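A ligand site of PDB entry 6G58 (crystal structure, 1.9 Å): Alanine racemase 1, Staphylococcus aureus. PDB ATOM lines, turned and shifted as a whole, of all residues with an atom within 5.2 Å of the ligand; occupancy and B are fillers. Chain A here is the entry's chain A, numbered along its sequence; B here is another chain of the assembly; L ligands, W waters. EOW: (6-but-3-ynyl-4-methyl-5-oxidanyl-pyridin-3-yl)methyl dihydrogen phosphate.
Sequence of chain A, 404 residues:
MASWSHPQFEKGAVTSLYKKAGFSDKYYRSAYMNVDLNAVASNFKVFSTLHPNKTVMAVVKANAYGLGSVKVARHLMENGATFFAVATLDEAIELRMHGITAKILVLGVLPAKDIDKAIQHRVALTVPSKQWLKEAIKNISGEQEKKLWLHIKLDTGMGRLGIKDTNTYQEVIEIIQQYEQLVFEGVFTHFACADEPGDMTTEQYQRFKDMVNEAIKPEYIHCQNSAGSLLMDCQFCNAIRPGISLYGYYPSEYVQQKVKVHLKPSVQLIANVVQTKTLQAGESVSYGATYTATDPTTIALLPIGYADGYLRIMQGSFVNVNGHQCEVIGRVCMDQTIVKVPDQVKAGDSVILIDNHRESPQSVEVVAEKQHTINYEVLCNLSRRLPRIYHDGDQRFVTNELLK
OH of Tyr 65 sits at hydrogen-bond distance from O1P of the ligand. The side-chain hydroxyl (OH) of Tyr 376 is in hydrogen-bond range of an oxygen (O3P) of the ligand, at 2.6 Å. The backbone NH (N) of Ile 244 lies within hydrogen-bond range of an oxygen (O1P) of the ligand (2.8 Å). The side-chain hydroxyl (OG) of Ser 226 sits at hydrogen-bond distance from an oxygen (O2P) of the ligand (2.6 Å). An oxygen (O2P) of the ligand lies within hydrogen-bond range of the backbone NH (N) of Gly 243, 3.0 Å away. The backbone NH of Ser 226 lies within hydrogen-bond range of an oxygen (O2P) of the ligand. A ring nitrogen (ND1) of His 190 lies close to a nitrogen (N1) of the ligand (3.4 Å). NE of Arg 241 sits at hydrogen-bond distance from N1 of the ligand (2.9 Å). C4A of the ligand is bonded to NZ of Lys 61 (1.3 Å).
A ring nitrogen (NE2) of His 190 lies within hydrogen-bond range of the side-chain hydroxyl (OH) of Tyr 287 of chain B, 2.7 Å away. The side-chain amino group (NZ) of Lys 61 lies within salt-bridge range of the side-chain carboxylate (OD2) of Asp 335 of chain B (3.7 Å). O of Pro 242 sits at hydrogen-bond distance from N of Val 59 (3.1 Å). The side-chain hydroxyl (OG) of Ser 226 is in hydrogen-bond range of the backbone NH (N) of Ile 244 (3.4 Å). The side-chain amide oxygen (OD1) of Asn 225 lies close to the backbone NH (N) of Ala 227 (3.5 Å). The side-chain amide oxygen (OE1) of Gln 336 of chain B sits at hydrogen-bond distance from the guanidinium group (NE) of Arg 160, at 3.3 Å. OG of Ser 226 is in hydrogen-bond range of N of Gly 243 (3.3 Å). The backbone NH of Ser 245 sits at hydrogen-bond distance from the side-chain hydroxyl of Ser 226, 3.1 Å away.
Water W2 lies within hydrogen-bond range of the side-chain hydroxyl (OH) of Tyr 287 of chain B (2.7 Å), an oxygen (O3) of the ligand (2.9 Å) and the guanidinium group (NH2) of Arg 160 (3.0 Å). Water W3 lies within hydrogen-bond range of an oxygen (O3P) of the ligand (2.9 Å), the side-chain amide nitrogen (ND2) of Asn 225 (3.0 Å), the side-chain hydroxyl (OH) of Tyr 287 of chain B (3.0 Å) and a ring nitrogen (NE2) of His 190 (3.5 Å). Water W1 lies within hydrogen-bond range of OD2 of Asp 335 of chain B and O3 of the ligand.
Val 59 touches the ligand (CG2 to C5A, 3.98 Å). O of Leu 107 touches C8 of the ligand (3.1 Å). CE of Lys 153 touches C8 of the ligand, at 3.4 Å. Arg 160 touches the ligand (NH2 to C1, 3.5 Å). Asn 225 touches the ligand. Pro 242 touches the ligand. Hydrophobic or aromatic side chains within 4 Å of the ligand: Val 59, Tyr 65, Leu 107, His 190, Ile 244 and Tyr 376. 14 residues have an atom within 4 Å of the ligand: Val 59, Lys 61, Tyr 65, Leu 107, Lys 153, Arg 160, His 190, Asn 225, Ser 226, Arg 241, Pro 242, Gly 243, Ile 244 and Tyr 376.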
ATOM      1  N   VAL A  59      -4.370 -16.397  -7.577  1.00  0.00           N
ATOM      2  CA  VAL A  59      -3.647 -17.550  -7.088  1.00  0.00           C
ATOM      3  C   VAL A  59      -4.395 -18.127  -5.891  1.00  0.00           C
ATOM      4  O   VAL A  59      -4.504 -17.488  -4.832  1.00  0.00           O
ATOM      5  CB  VAL A  59      -2.201 -17.186  -6.703  1.00  0.00           C
ATOM      6  CG1 VAL A  59      -1.463 -18.416  -6.186  1.00  0.00           C
ATOM      7  CG2 VAL A  59      -1.499 -16.638  -7.933  1.00  0.00           C
ATOM      8  N   LYS A  61      -3.835 -21.471  -4.864  1.00  0.00           N
ATOM      9  CA  LYS A  61      -3.084 -22.650  -4.398  1.00  0.00           C
ATOM     10  C   LYS A  61      -3.257 -22.835  -2.877  1.00  0.00           C
ATOM     11  O   LYS A  61      -3.633 -21.905  -2.145  1.00  0.00           O
ATOM     12  CB  LYS A  61      -1.596 -22.544  -4.777  1.00  0.00           C
ATOM     13  CG  LYS A  61      -0.760 -21.564  -3.933  1.00  0.00           C
ATOM     14  CD  LYS A  61       0.560 -21.212  -4.599  1.00  0.00           C
ATOM     15  CE  LYS A  61       1.631 -20.550  -3.689  1.00  0.00           C
ATOM     16  NZ  LYS A  61       2.302 -19.876  -4.732  1.00  0.00           N
ATOM     17  N   TYR A  65      -4.780 -20.449   0.385  1.00  0.00           N
ATOM     18  CA  TYR A  65      -3.963 -20.059   1.528  1.00  0.00           C
ATOM     19  C   TYR A  65      -4.766 -20.317   2.840  1.00  0.00           C
ATOM     20  O   TYR A  65      -4.656 -19.589   3.814  1.00  0.00           O
ATOM     21  CB  TYR A  65      -3.492 -18.603   1.431  1.00  0.00           C
ATOM     22  CG  TYR A  65      -2.496 -18.240   0.325  1.00  0.00           C
ATOM     23  CD1 TYR A  65      -2.635 -18.743  -0.954  1.00  0.00           C
ATOM     24  CD2 TYR A  65      -1.496 -17.314   0.537  1.00  0.00           C
ATOM     25  CE1 TYR A  65      -1.765 -18.379  -1.967  1.00  0.00           C
ATOM     26  CE2 TYR A  65      -0.607 -16.964  -0.481  1.00  0.00           C
ATOM     27  CZ  TYR A  65      -0.753 -17.491  -1.742  1.00  0.00           C
ATOM     28  OH  TYR A  65       0.044 -17.199  -2.828  1.00  0.00           O
ATOM     29  N   LEU A 107       0.905 -24.498 -11.557  1.00  0.00           N
ATOM     30  CA  LEU A 107       2.224 -23.862 -11.446  1.00  0.00           C
ATOM     31  C   LEU A 107       3.380 -24.839 -11.162  1.00  0.00           C
ATOM     32  O   LEU A 107       4.532 -24.535 -11.482  1.00  0.00           O
ATOM     33  CB  LEU A 107       2.203 -22.827 -10.325  1.00  0.00           C
ATOM     34  CG  LEU A 107       1.203 -21.697 -10.520  1.00  0.00           C
ATOM     35  CD1 LEU A 107       1.012 -20.972  -9.200  1.00  0.00           C
ATOM     36  CD2 LEU A 107       1.623 -20.750 -11.657  1.00  0.00           C
ATOM     37  N   GLY A 108       3.062 -25.981 -10.533  1.00  0.00           N
ATOM     38  CA  GLY A 108       4.044 -27.041 -10.322  1.00  0.00           C
ATOM     39  C   GLY A 108       4.229 -27.903 -11.556  1.00  0.00           C
ATOM     40  O   GLY A 108       3.505 -27.755 -12.541  1.00  0.00           O
ATOM     41  N   LYS A 153       7.754 -21.883 -18.307  1.00  0.00           N
ATOM     42  CA  LYS A 153       8.315 -21.193 -17.165  1.00  0.00           C
ATOM     43  C   LYS A 153       9.789 -20.889 -17.435  1.00  0.00           C
ATOM     44  O   LYS A 153      10.588 -21.801 -17.736  1.00  0.00           O
ATOM     45  CB  LYS A 153       8.194 -22.070 -15.925  1.00  0.00           C
ATOM     46  CG  LYS A 153       8.656 -21.394 -14.645  1.00  0.00           C
ATOM     47  CD  LYS A 153       8.665 -22.479 -13.550  1.00  0.00           C
ATOM     48  CE  LYS A 153       9.001 -21.960 -12.176  1.00  0.00           C
ATOM     49  NZ  LYS A 153       9.259 -23.116 -11.242  1.00  0.00           N
ATOM     50  N   ARG A 160      14.620 -22.102  -9.125  1.00  0.00           N
ATOM     51  CA  ARG A 160      13.922 -23.396  -8.985  1.00  0.00           C
ATOM     52  C   ARG A 160      13.876 -24.009 -10.385  1.00  0.00           C
ATOM     53  O   ARG A 160      14.845 -23.852 -11.167  1.00  0.00           O
ATOM     54  CB  ARG A 160      12.564 -23.216  -8.286  1.00  0.00           C
ATOM     55  CG  ARG A 160      12.725 -22.673  -6.865  1.00  0.00           C
ATOM     56  CD  ARG A 160      11.420 -22.542  -6.089  1.00  0.00           C
ATOM     57  NE  ARG A 160      10.393 -21.810  -6.850  1.00  0.00           N
ATOM     58  CZ  ARG A 160       9.129 -21.588  -6.442  1.00  0.00           C
ATOM     59  NH1 ARG A 160       8.692 -22.004  -5.260  1.00  0.00           N
ATOM     60  NH2 ARG A 160       8.292 -20.935  -7.226  1.00  0.00           N
ATOM     61  N   PHE A 188       6.022 -17.259 -18.495  1.00  0.00           N
ATOM     62  CA  PHE A 188       6.097 -16.601 -17.229  1.00  0.00           C
ATOM     63  C   PHE A 188       7.420 -16.804 -16.495  1.00  0.00           C
ATOM     64  O   PHE A 188       8.214 -17.689 -16.828  1.00  0.00           O
ATOM     65  CB  PHE A 188       4.892 -17.014 -16.353  1.00  0.00           C
ATOM     66  CG  PHE A 188       4.947 -18.388 -15.751  1.00  0.00           C
ATOM     67  CD1 PHE A 188       4.576 -19.498 -16.474  1.00  0.00           C
ATOM     68  CD2 PHE A 188       5.223 -18.567 -14.402  1.00  0.00           C
ATOM     69  CE1 PHE A 188       4.535 -20.774 -15.891  1.00  0.00           C
ATOM     70  CE2 PHE A 188       5.168 -19.828 -13.778  1.00  0.00           C
ATOM     71  CZ  PHE A 188       4.833 -20.933 -14.535  1.00  0.00           C
ATOM     72  N   HIS A 190       9.057 -15.723 -12.194  1.00  0.00           N
ATOM     73  CA  HIS A 190       8.679 -15.458 -10.802  1.00  0.00           C
ATOM     74  C   HIS A 190       9.810 -14.734 -10.093  1.00  0.00           C
ATOM     75  O   HIS A 190      10.973 -15.106 -10.242  1.00  0.00           O
ATOM     76  CB  HIS A 190       8.375 -16.764 -10.094  1.00  0.00           C
ATOM     77  CG  HIS A 190       7.672 -16.616  -8.779  1.00  0.00           C
ATOM     78  ND1 HIS A 190       6.476 -15.943  -8.630  1.00  0.00           N
ATOM     79  CD2 HIS A 190       7.959 -17.132  -7.563  1.00  0.00           C
ATOM     80  CE1 HIS A 190       6.081 -16.009  -7.357  1.00  0.00           C
ATOM     81  NE2 HIS A 190       6.960 -16.743  -6.696  1.00  0.00           N
ATOM     82  N   ASN A 225       3.840 -11.458  -8.777  1.00  0.00           N
ATOM     83  CA  ASN A 225       3.133 -11.915  -7.574  1.00  0.00           C
ATOM     84  C   ASN A 225       2.483 -10.690  -6.900  1.00  0.00           C
ATOM     85  O   ASN A 225       2.406  -9.605  -7.527  1.00  0.00           O
ATOM     86  CB  ASN A 225       4.076 -12.711  -6.643  1.00  0.00           C
ATOM     87  CG  ASN A 225       5.330 -11.938  -6.237  1.00  0.00           C
ATOM     88  OD1 ASN A 225       5.481 -10.763  -6.579  1.00  0.00           O
ATOM     89  ND2 ASN A 225       6.264 -12.612  -5.552  1.00  0.00           N
ATOM     90  N   SER A 226       1.991 -10.819  -5.667  1.00  0.00           N
ATOM     91  CA  SER A 226       1.373  -9.668  -4.982  1.00  0.00           C
ATOM     92  C   SER A 226       2.337  -8.480  -4.915  1.00  0.00           C
ATOM     93  O   SER A 226       1.968  -7.337  -5.216  1.00  0.00           O
ATOM     94  CB  SER A 226       0.915 -10.055  -3.545  1.00  0.00           C
ATOM     95  OG  SER A 226      -0.143 -10.994  -3.554  1.00  0.00           O
ATOM     96  N   ALA A 227       3.563  -8.752  -4.475  1.00  0.00           N
ATOM     97  CA  ALA A 227       4.557  -7.691  -4.296  1.00  0.00           C
ATOM     98  C   ALA A 227       4.868  -6.997  -5.620  1.00  0.00           C
ATOM     99  O   ALA A 227       4.883  -5.773  -5.729  1.00  0.00           O
ATOM    100  CB  ALA A 227       5.824  -8.247  -3.673  1.00  0.00           C
ATOM    101  N   ARG A 241      -0.314 -12.370 -11.128  1.00  0.00           N
ATOM    102  CA  ARG A 241      -0.608 -13.548 -10.291  1.00  0.00           C
ATOM    103  C   ARG A 241      -0.567 -13.193  -8.804  1.00  0.00           C
ATOM    104  O   ARG A 241       0.308 -13.663  -8.096  1.00  0.00           O
ATOM    105  CB  ARG A 241       0.411 -14.651 -10.552  1.00  0.00           C
ATOM    106  CG  ARG A 241       0.506 -15.173 -11.951  1.00  0.00           C
ATOM    107  CD  ARG A 241       1.321 -16.478 -11.975  1.00  0.00           C
ATOM    108  NE  ARG A 241       2.647 -16.310 -11.395  1.00  0.00           N
ATOM    109  CZ  ARG A 241       3.705 -15.772 -11.979  1.00  0.00           C
ATOM    110  NH1 ARG A 241       3.665 -15.341 -13.234  1.00  0.00           N
ATOM    111  NH2 ARG A 241       4.845 -15.654 -11.298  1.00  0.00           N
ATOM    112  N   PRO A 242      -1.510 -12.373  -8.328  1.00  0.00           N
ATOM    113  CA  PRO A 242      -1.546 -12.095  -6.886  1.00  0.00           C
ATOM    114  C   PRO A 242      -2.174 -13.242  -6.107  1.00  0.00           C
ATOM    115  O   PRO A 242      -3.219 -13.766  -6.525  1.00  0.00           O
ATOM    116  CB  PRO A 242      -2.432 -10.857  -6.805  1.00  0.00           C
ATOM    117  CG  PRO A 242      -3.398 -11.062  -7.921  1.00  0.00           C
ATOM    118  CD  PRO A 242      -2.578 -11.678  -9.032  1.00  0.00           C
ATOM    119  N   GLY A 243      -1.551 -13.601  -5.005  1.00  0.00           N
ATOM    120  CA  GLY A 243      -2.069 -14.553  -4.034  1.00  0.00           C
ATOM    121  C   GLY A 243      -2.380 -13.868  -2.717  1.00  0.00           C
ATOM    122  O   GLY A 243      -3.512 -13.439  -2.490  1.00  0.00           O
ATOM    123  N   ILE A 244      -1.383 -13.722  -1.848  1.00  0.00           N
ATOM    124  CA  ILE A 244      -1.654 -13.312  -0.476  1.00  0.00           C
ATOM    125  C   ILE A 244      -2.401 -11.985  -0.343  1.00  0.00           C
ATOM    126  O   ILE A 244      -3.229 -11.824   0.573  1.00  0.00           O
ATOM    127  CB  ILE A 244      -0.388 -13.298   0.421  1.00  0.00           C
ATOM    128  CG1 ILE A 244      -0.829 -13.507   1.901  1.00  0.00           C
ATOM    129  CG2 ILE A 244       0.488 -12.095   0.120  1.00  0.00           C
ATOM    130  CD1 ILE A 244       0.269 -13.461   2.889  1.00  0.00           C
ATOM    131  N   SER A 245      -2.135 -11.026  -1.243  1.00  0.00           N
ATOM    132  CA  SER A 245      -2.817  -9.766  -1.146  1.00  0.00           C
ATOM    133  C   SER A 245      -4.293  -9.812  -1.580  1.00  0.00           C
ATOM    134  O   SER A 245      -5.065  -8.947  -1.174  1.00  0.00           O
ATOM    135  CB  SER A 245      -2.041  -8.672  -1.886  1.00  0.00           C
ATOM    136  OG  SER A 245      -0.820  -8.433  -1.204  1.00  0.00           O
ATOM    137  N   PRO A 251       2.585  -8.579   1.423  1.00  0.00           N
ATOM    138  CA  PRO A 251       3.615  -9.634   1.423  1.00  0.00           C
ATOM    139  C   PRO A 251       4.744  -9.387   2.361  1.00  0.00           C
ATOM    140  O   PRO A 251       5.418 -10.319   2.737  1.00  0.00           O
ATOM    141  CB  PRO A 251       4.115  -9.684  -0.018  1.00  0.00           C
ATOM    142  CG  PRO A 251       3.467  -8.586  -0.739  1.00  0.00           C
ATOM    143  CD  PRO A 251       2.422  -7.949   0.106  1.00  0.00           C
ATOM    144  N   TYR A 376       2.057 -15.889   5.500  1.00  0.00           N
ATOM    145  CA  TYR A 376       1.693 -17.017   4.628  1.00  0.00           C
ATOM    146  C   TYR A 376       1.552 -18.339   5.408  1.00  0.00           C
ATOM    147  O   TYR A 376       0.572 -19.101   5.199  1.00  0.00           O
ATOM    148  CB  TYR A 376       2.737 -17.261   3.539  1.00  0.00           C
ATOM    149  CG  TYR A 376       3.004 -16.132   2.530  1.00  0.00           C
ATOM    150  CD1 TYR A 376       3.858 -15.063   2.849  1.00  0.00           C
ATOM    151  CD2 TYR A 376       2.497 -16.204   1.248  1.00  0.00           C
ATOM    152  CE1 TYR A 376       4.116 -14.061   1.907  1.00  0.00           C
ATOM    153  CE2 TYR A 376       2.776 -15.223   0.306  1.00  0.00           C
ATOM    154  CZ  TYR A 376       3.593 -14.143   0.647  1.00  0.00           C
ATOM    155  OH  TYR A 376       3.847 -13.199  -0.326  1.00  0.00           O
ATOM    156  N   TYR B 287      13.241 -17.789  -2.259  1.00  0.00           N
ATOM    157  CA  TYR B 287      12.867 -16.422  -1.815  1.00  0.00           C
ATOM    158  C   TYR B 287      13.945 -15.814  -0.930  1.00  0.00           C
ATOM    159  O   TYR B 287      14.491 -16.488  -0.074  1.00  0.00           O
ATOM    160  CB  TYR B 287      11.541 -16.420  -1.043  1.00  0.00           C
ATOM    161  CG  TYR B 287      10.317 -16.754  -1.880  1.00  0.00           C
ATOM    162  CD1 TYR B 287       9.867 -15.883  -2.891  1.00  0.00           C
ATOM    163  CD2 TYR B 287       9.591 -17.960  -1.661  1.00  0.00           C
ATOM    164  CE1 TYR B 287       8.748 -16.183  -3.643  1.00  0.00           C
ATOM    165  CE2 TYR B 287       8.461 -18.261  -2.412  1.00  0.00           C
ATOM    166  CZ  TYR B 287       8.044 -17.372  -3.404  1.00  0.00           C
ATOM    167  OH  TYR B 287       6.927 -17.661  -4.140  1.00  0.00           O
ATOM    168  N   ASP B 335       4.890 -24.633  -1.645  1.00  0.00           N
ATOM    169  CA  ASP B 335       4.688 -25.864  -2.394  1.00  0.00           C
ATOM    170  C   ASP B 335       5.953 -26.576  -2.873  1.00  0.00           C
ATOM    171  O   ASP B 335       5.829 -27.620  -3.508  1.00  0.00           O
ATOM    172  CB  ASP B 335       3.811 -25.556  -3.631  1.00  0.00           C
ATOM    173  CG  ASP B 335       2.690 -24.575  -3.317  1.00  0.00           C
ATOM    174  OD1 ASP B 335       1.865 -24.852  -2.398  1.00  0.00           O
ATOM    175  OD2 ASP B 335       2.646 -23.519  -3.991  1.00  0.00           O
ATOM    176  N   GLN B 336       7.131 -26.020  -2.572  1.00  0.00           N
ATOM    177  CA  GLN B 336       8.393 -26.517  -3.130  1.00  0.00           C
ATOM    178  C   GLN B 336       9.515 -26.399  -2.111  1.00  0.00           C
ATOM    179  O   GLN B 336       9.543 -25.443  -1.324  1.00  0.00           O
ATOM    180  CB  GLN B 336       8.771 -25.774  -4.412  1.00  0.00           C
ATOM    181  CG  GLN B 336       7.765 -26.000  -5.533  1.00  0.00           C
ATOM    182  CD  GLN B 336       8.156 -25.313  -6.864  1.00  0.00           C
ATOM    183  OE1 GLN B 336       9.315 -24.921  -7.075  1.00  0.00           O
ATOM    184  NE2 GLN B 336       7.182 -25.197  -7.763  1.00  0.00           N
HETATM  185  O3P EOW L   1       3.280 -13.641  -2.834  1.00  0.00           O
HETATM  186  P   EOW L   1       2.045 -14.156  -3.489  1.00  0.00           P
HETATM  187  O1P EOW L   1       1.050 -14.819  -2.516  1.00  0.00           O
HETATM  188  O2P EOW L   1       1.274 -13.054  -4.220  1.00  0.00           O
HETATM  189  O4P EOW L   1       2.526 -15.220  -4.587  1.00  0.00           O
HETATM  190  C5A EOW L   1       1.581 -15.719  -5.584  1.00  0.00           C
HETATM  191  C5  EOW L   1       2.290 -16.678  -6.519  1.00  0.00           C
HETATM  192  C6  EOW L   1       2.619 -16.263  -7.807  1.00  0.00           C
HETATM  193  N1  EOW L   1       3.266 -17.053  -8.681  1.00  0.00           N
HETATM  194  C4  EOW L   1       2.741 -18.030  -6.093  1.00  0.00           C
HETATM  195  C4A EOW L   1       2.329 -18.605  -4.827  1.00  0.00           C
HETATM  196  C3  EOW L   1       3.408 -18.884  -7.097  1.00  0.00           C
HETATM  197  O3  EOW L   1       3.820 -20.137  -6.786  1.00  0.00           O
HETATM  198  C2  EOW L   1       3.702 -18.306  -8.410  1.00  0.00           C
HETATM  199  C2A EOW L   1       4.389 -19.100  -9.472  1.00  0.00           C
HETATM  200  C1  EOW L   1       5.791 -19.611  -9.211  1.00  0.00           C
HETATM  201  C7  EOW L   1       5.941 -20.901  -9.911  1.00  0.00           C
HETATM  202  C8  EOW L   1       6.055 -22.019 -10.516  1.00  0.00           C
HETATM  203  O   HOH W   1       3.239 -23.177  -6.431  1.00  0.00           O
HETATM  204  O   HOH W   2       6.262 -20.035  -5.240  1.00  0.00           O
HETATM  205  O   HOH W   3       5.527 -15.043  -4.048  1.00  0.00           O
HETATM  206  O   HOH W   4       4.335 -11.138  -3.162  1.00  0.00           O
